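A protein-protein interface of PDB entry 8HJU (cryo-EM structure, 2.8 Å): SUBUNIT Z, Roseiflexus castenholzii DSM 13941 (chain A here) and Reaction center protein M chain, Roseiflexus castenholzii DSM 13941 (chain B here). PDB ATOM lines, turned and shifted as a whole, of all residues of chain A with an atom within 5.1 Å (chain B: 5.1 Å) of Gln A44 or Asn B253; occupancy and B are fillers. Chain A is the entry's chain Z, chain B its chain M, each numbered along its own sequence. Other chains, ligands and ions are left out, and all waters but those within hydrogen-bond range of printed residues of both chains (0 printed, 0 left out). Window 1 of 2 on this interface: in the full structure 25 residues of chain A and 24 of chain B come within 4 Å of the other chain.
Gln A44 touches just these residues of chain B: Asn B250 (3.5 Å) and Asn B253 (3.4 Å).
Of the printed residues of chain B, Ala A45 touches Ala B249 and Asn B250.
Ser B251 touches none of the printed residues of chain A.
Asn B253 touches just these residues of chain A: Thr A41 and Gln A44.
His B255 touches none of the printed residues of chain A.
Of the printed residues of chain A, Trp B257 touches Thr A41 (2.6 Å).
The nearest printed residue of chain B that does not touch Gln A44 is Tyr B252 (5.8 Å).
The nearest residue of chain A that does not touch Asn B253 is Ala A45 (4.05 Å).
Thr A41 touches Ala B249.
Gln A44 touches Asn B250.
Gln A44 touches Asn B253 (CB to OD1, 3.4 Å).
CB of Ala A45 touches C of Ala B249 (3.5 Å).
CB of Ala A45 touches N of Asn B250, at 3.6 Å.
CB of Asn B250 touches OH of Tyr A49, 3.2 Å away.
The backbone carbonyl oxygen (O) of Thr A41 lies close to the side-chain amide oxygen (OD1) of Asn B253, at 3.0 Å.
The indole nitrogen of Trp B257 lies within hydrogen-bond range of the side-chain hydroxyl of Thr A41, 2.6 Å away.
OD1 of Asn B250 is in hydrogen-bond range of N of Tyr B252 (2.8 Å).
The side-chain amide oxygen (OD1) of Asn B250 is in hydrogen-bond range of the backbone NH (N) of Asn B253, at 2.8 Å.
OG of Ser A47 sits at hydrogen-bond distance from O of Gln A44 (2.7 Å).
The backbone carbonyl oxygen (O) of Ala A45 is in hydrogen-bond range of the side-chain hydroxyl (OH) of Tyr A49 (3.3 Å).
Hydrophobic or aromatic side chains of chain B that line the printed part of chain A: Ala B249 and Trp B257.
Printed residues of chain A that touch a printed residue of chain B: Thr A41, Gln A44, Ala A45 and Tyr A49.
Hydrophobic or aromatic side chains of chain A that line the printed part of chain B: Ala A45 and Tyr A49.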
ATOM      1  N   PHE A  40      11.903  22.646  13.949  1.00  0.00           N
ATOM      2  CA  PHE A  40      11.107  23.562  14.756  1.00  0.00           C
ATOM      3  C   PHE A  40      10.212  24.448  13.906  1.00  0.00           C
ATOM      4  O   PHE A  40       9.087  24.766  14.318  1.00  0.00           O
ATOM      5  CB  PHE A  40      12.027  24.382  15.651  1.00  0.00           C
ATOM      6  CG  PHE A  40      12.454  23.641  16.872  1.00  0.00           C
ATOM      7  CD1 PHE A  40      11.545  23.339  17.868  1.00  0.00           C
ATOM      8  CD2 PHE A  40      13.749  23.203  17.007  1.00  0.00           C
ATOM      9  CE1 PHE A  40      11.934  22.640  18.986  1.00  0.00           C
ATOM     10  CE2 PHE A  40      14.140  22.504  18.113  1.00  0.00           C
ATOM     11  CZ  PHE A  40      13.236  22.222  19.106  1.00  0.00           C
ATOM     12  N   THR A  41      10.674  24.812  12.711  1.00  0.00           N
ATOM     13  CA  THR A  41       9.812  25.460  11.741  1.00  0.00           C
ATOM     14  C   THR A  41       8.533  24.668  11.554  1.00  0.00           C
ATOM     15  O   THR A  41       7.434  25.218  11.663  1.00  0.00           O
ATOM     16  CB  THR A  41      10.548  25.598  10.407  1.00  0.00           C
ATOM     17  OG1 THR A  41      11.739  26.365  10.589  1.00  0.00           O
ATOM     18  CG2 THR A  41       9.693  26.277   9.378  1.00  0.00           C
ATOM     19  N   ASP A  42       8.649  23.362  11.337  1.00  0.00           N
ATOM     20  CA  ASP A  42       7.437  22.610  11.073  1.00  0.00           C
ATOM     21  C   ASP A  42       6.677  22.248  12.336  1.00  0.00           C
ATOM     22  O   ASP A  42       5.460  22.081  12.276  1.00  0.00           O
ATOM     23  CB  ASP A  42       7.723  21.352  10.273  1.00  0.00           C
ATOM     24  CG  ASP A  42       6.507  20.907   9.493  1.00  0.00           C
ATOM     25  OD1 ASP A  42       5.466  21.578   9.628  1.00  0.00           O
ATOM     26  OD2 ASP A  42       6.576  19.917   8.743  1.00  0.00           O
ATOM     27  N   LYS A  43       7.337  22.086  13.479  1.00  0.00           N
ATOM     28  CA  LYS A  43       6.543  21.960  14.693  1.00  0.00           C
ATOM     29  C   LYS A  43       5.609  23.147  14.846  1.00  0.00           C
ATOM     30  O   LYS A  43       4.410  22.973  15.102  1.00  0.00           O
ATOM     31  CB  LYS A  43       7.440  21.821  15.911  1.00  0.00           C
ATOM     32  CG  LYS A  43       7.662  20.395  16.308  1.00  0.00           C
ATOM     33  CD  LYS A  43       7.514  20.231  17.790  1.00  0.00           C
ATOM     34  CE  LYS A  43       8.098  21.415  18.503  1.00  0.00           C
ATOM     35  NZ  LYS A  43       8.061  21.226  19.970  1.00  0.00           N
ATOM     36  N   GLN A  44       6.124  24.360  14.646  1.00  0.00           N
ATOM     37  CA  GLN A  44       5.259  25.528  14.738  1.00  0.00           C
ATOM     38  C   GLN A  44       4.219  25.539  13.626  1.00  0.00           C
ATOM     39  O   GLN A  44       3.047  25.832  13.873  1.00  0.00           O
ATOM     40  CB  GLN A  44       6.092  26.806  14.719  1.00  0.00           C
ATOM     41  CG  GLN A  44       5.299  28.093  14.889  1.00  0.00           C
ATOM     42  CD  GLN A  44       4.268  28.035  16.000  1.00  0.00           C
ATOM     43  OE1 GLN A  44       4.377  27.219  16.907  1.00  0.00           O
ATOM     44  NE2 GLN A  44       3.253  28.882  15.923  1.00  0.00           N
ATOM     45  N   ALA A  45       4.618  25.204  12.399  1.00  0.00           N
ATOM     46  CA  ALA A  45       3.697  25.327  11.277  1.00  0.00           C
ATOM     47  C   ALA A  45       2.578  24.296  11.325  1.00  0.00           C
ATOM     48  O   ALA A  45       1.474  24.568  10.849  1.00  0.00           O
ATOM     49  CB  ALA A  45       4.459  25.213   9.964  1.00  0.00           C
ATOM     50  N   THR A  46       2.834  23.111  11.869  1.00  0.00           N
ATOM     51  CA  THR A  46       1.823  22.074  11.965  1.00  0.00           C
ATOM     52  C   THR A  46       1.138  22.040  13.317  1.00  0.00           C
ATOM     53  O   THR A  46       0.243  21.217  13.516  1.00  0.00           O
ATOM     54  CB  THR A  46       2.433  20.701  11.680  1.00  0.00           C
ATOM     55  OG1 THR A  46       3.514  20.463  12.586  1.00  0.00           O
ATOM     56  CG2 THR A  46       2.935  20.627  10.259  1.00  0.00           C
ATOM     57  N   SER A  47       1.533  22.898  14.253  1.00  0.00           N
ATOM     58  CA  SER A  47       0.763  23.001  15.480  1.00  0.00           C
ATOM     59  C   SER A  47      -0.621  23.578  15.188  1.00  0.00           C
ATOM     60  O   SER A  47      -0.918  24.036  14.084  1.00  0.00           O
ATOM     61  CB  SER A  47       1.498  23.857  16.504  1.00  0.00           C
ATOM     62  OG  SER A  47       1.633  25.186  16.049  1.00  0.00           O
ATOM     63  N   TYR A  49      -3.342  26.378  15.693  1.00  0.00           N
ATOM     64  CA  TYR A  49      -3.504  27.779  16.033  1.00  0.00           C
ATOM     65  C   TYR A  49      -4.653  28.328  15.203  1.00  0.00           C
ATOM     66  O   TYR A  49      -5.274  27.611  14.420  1.00  0.00           O
ATOM     67  CB  TYR A  49      -2.208  28.558  15.814  1.00  0.00           C
ATOM     68  CG  TYR A  49      -1.524  28.302  14.497  1.00  0.00           C
ATOM     69  CD1 TYR A  49      -2.056  28.780  13.319  1.00  0.00           C
ATOM     70  CD2 TYR A  49      -0.333  27.610  14.439  1.00  0.00           C
ATOM     71  CE1 TYR A  49      -1.438  28.564  12.130  1.00  0.00           C
ATOM     72  CE2 TYR A  49       0.293  27.389  13.250  1.00  0.00           C
ATOM     73  CZ  TYR A  49      -0.263  27.868  12.097  1.00  0.00           C
ATOM     74  OH  TYR A  49       0.355  27.654  10.894  1.00  0.00           O
ATOM     75  N   ALA B 249       6.584  25.824   6.532  1.00  0.00           N
ATOM     76  CA  ALA B 249       6.586  26.921   7.481  1.00  0.00           C
ATOM     77  C   ALA B 249       5.215  27.577   7.469  1.00  0.00           C
ATOM     78  O   ALA B 249       4.398  27.319   6.587  1.00  0.00           O
ATOM     79  CB  ALA B 249       7.663  27.947   7.132  1.00  0.00           C
ATOM     80  N   ASN B 250       4.947  28.404   8.467  1.00  0.00           N
ATOM     81  CA  ASN B 250       3.718  29.179   8.467  1.00  0.00           C
ATOM     82  C   ASN B 250       3.999  30.603   7.986  1.00  0.00           C
ATOM     83  O   ASN B 250       5.054  30.906   7.429  1.00  0.00           O
ATOM     84  CB  ASN B 250       3.037  29.136   9.835  1.00  0.00           C
ATOM     85  CG  ASN B 250       3.872  29.731  10.935  1.00  0.00           C
ATOM     86  OD1 ASN B 250       4.774  30.523  10.698  1.00  0.00           O
ATOM     87  ND2 ASN B 250       3.562  29.358  12.164  1.00  0.00           N
ATOM     88  N   SER B 251       3.024  31.488   8.185  1.00  0.00           N
ATOM     89  CA  SER B 251       3.157  32.878   7.772  1.00  0.00           C
ATOM     90  C   SER B 251       4.277  33.599   8.508  1.00  0.00           C
ATOM     91  O   SER B 251       4.749  34.640   8.044  1.00  0.00           O
ATOM     92  CB  SER B 251       1.838  33.603   8.009  1.00  0.00           C
ATOM     93  OG  SER B 251       1.026  33.549   6.859  1.00  0.00           O
ATOM     94  N   TYR B 252       4.705  33.082   9.656  1.00  0.00           N
ATOM     95  CA  TYR B 252       5.667  33.791  10.490  1.00  0.00           C
ATOM     96  C   TYR B 252       7.079  33.229  10.373  1.00  0.00           C
ATOM     97  O   TYR B 252       8.040  33.997  10.305  1.00  0.00           O
ATOM     98  CB  TYR B 252       5.196  33.760  11.947  1.00  0.00           C
ATOM     99  CG  TYR B 252       6.156  34.365  12.937  1.00  0.00           C
ATOM    100  CD1 TYR B 252       6.433  35.720  12.929  1.00  0.00           C
ATOM    101  CD2 TYR B 252       6.775  33.579  13.893  1.00  0.00           C
ATOM    102  CE1 TYR B 252       7.302  36.269  13.834  1.00  0.00           C
ATOM    103  CE2 TYR B 252       7.645  34.119  14.802  1.00  0.00           C
ATOM    104  CZ  TYR B 252       7.907  35.464  14.769  1.00  0.00           C
ATOM    105  OH  TYR B 252       8.779  36.002  15.683  1.00  0.00           O
ATOM    106  N   ASN B 253       7.219  31.901  10.337  1.00  0.00           N
ATOM    107  CA  ASN B 253       8.538  31.272  10.326  1.00  0.00           C
ATOM    108  C   ASN B 253       9.329  31.635   9.080  1.00  0.00           C
ATOM    109  O   ASN B 253      10.554  31.813   9.136  1.00  0.00           O
ATOM    110  CB  ASN B 253       8.391  29.754  10.403  1.00  0.00           C
ATOM    111  CG  ASN B 253       7.857  29.288  11.717  1.00  0.00           C
ATOM    112  OD1 ASN B 253       7.219  28.247  11.803  1.00  0.00           O
ATOM    113  ND2 ASN B 253       8.111  30.058  12.760  1.00  0.00           N
ATOM    114  N   ILE B 254       8.650  31.714   7.936  1.00  0.00           N
ATOM    115  CA  ILE B 254       9.346  31.855   6.665  1.00  0.00           C
ATOM    116  C   ILE B 254      10.130  33.154   6.624  1.00  0.00           C
ATOM    117  O   ILE B 254      11.206  33.227   6.019  1.00  0.00           O
ATOM    118  CB  ILE B 254       8.339  31.733   5.505  1.00  0.00           C
ATOM    119  CG1 ILE B 254       9.070  31.645   4.172  1.00  0.00           C
ATOM    120  CG2 ILE B 254       7.321  32.858   5.530  1.00  0.00           C
ATOM    121  CD1 ILE B 254       9.948  30.452   4.078  1.00  0.00           C
ATOM    122  N   HIS B 255       9.650  34.179   7.318  1.00  0.00           N
ATOM    123  CA  HIS B 255      10.358  35.445   7.330  1.00  0.00           C
ATOM    124  C   HIS B 255      11.533  35.427   8.293  1.00  0.00           C
ATOM    125  O   HIS B 255      12.530  36.116   8.054  1.00  0.00           O
ATOM    126  CB  HIS B 255       9.372  36.560   7.641  1.00  0.00           C
ATOM    127  CG  HIS B 255       8.223  36.599   6.687  1.00  0.00           C
ATOM    128  ND1 HIS B 255       7.018  35.987   6.948  1.00  0.00           N
ATOM    129  CD2 HIS B 255       8.114  37.128   5.449  1.00  0.00           C
ATOM    130  CE1 HIS B 255       6.207  36.165   5.924  1.00  0.00           C
ATOM    131  NE2 HIS B 255       6.847  36.855   5.001  1.00  0.00           N
ATOM    132  N   ILE B 256      11.458  34.623   9.354  1.00  0.00           N
ATOM    133  CA  ILE B 256      12.646  34.343  10.154  1.00  0.00           C
ATOM    134  C   ILE B 256      13.719  33.700   9.286  1.00  0.00           C
ATOM    135  O   ILE B 256      14.895  34.085   9.327  1.00  0.00           O
ATOM    136  CB  ILE B 256      12.293  33.446  11.351  1.00  0.00           C
ATOM    137  CG1 ILE B 256      11.142  34.042  12.150  1.00  0.00           C
ATOM    138  CG2 ILE B 256      13.498  33.251  12.234  1.00  0.00           C
ATOM    139  CD1 ILE B 256      10.606  33.117  13.193  1.00  0.00           C
ATOM    140  N   TRP B 257      13.325  32.706   8.489  1.00  0.00           N
ATOM    141  CA  TRP B 257      14.269  32.065   7.578  1.00  0.00           C
ATOM    142  C   TRP B 257      14.892  33.081   6.632  1.00  0.00           C
ATOM    143  O   TRP B 257      16.108  33.083   6.417  1.00  0.00           O
ATOM    144  CB  TRP B 257      13.566  30.970   6.781  1.00  0.00           C
ATOM    145  CG  TRP B 257      13.423  29.682   7.500  1.00  0.00           C
ATOM    146  CD1 TRP B 257      12.406  29.314   8.315  1.00  0.00           C
ATOM    147  CD2 TRP B 257      14.322  28.574   7.453  1.00  0.00           C
ATOM    148  NE1 TRP B 257      12.613  28.048   8.790  1.00  0.00           N
ATOM    149  CE2 TRP B 257      13.786  27.570   8.273  1.00  0.00           C
ATOM    150  CE3 TRP B 257      15.531  28.336   6.799  1.00  0.00           C
ATOM    151  CZ2 TRP B 257      14.412  26.348   8.455  1.00  0.00           C
ATOM    152  CZ3 TRP B 257      16.151  27.125   6.984  1.00  0.00           C
ATOM    153  CH2 TRP B 257      15.591  26.146   7.802  1.00  0.00           C
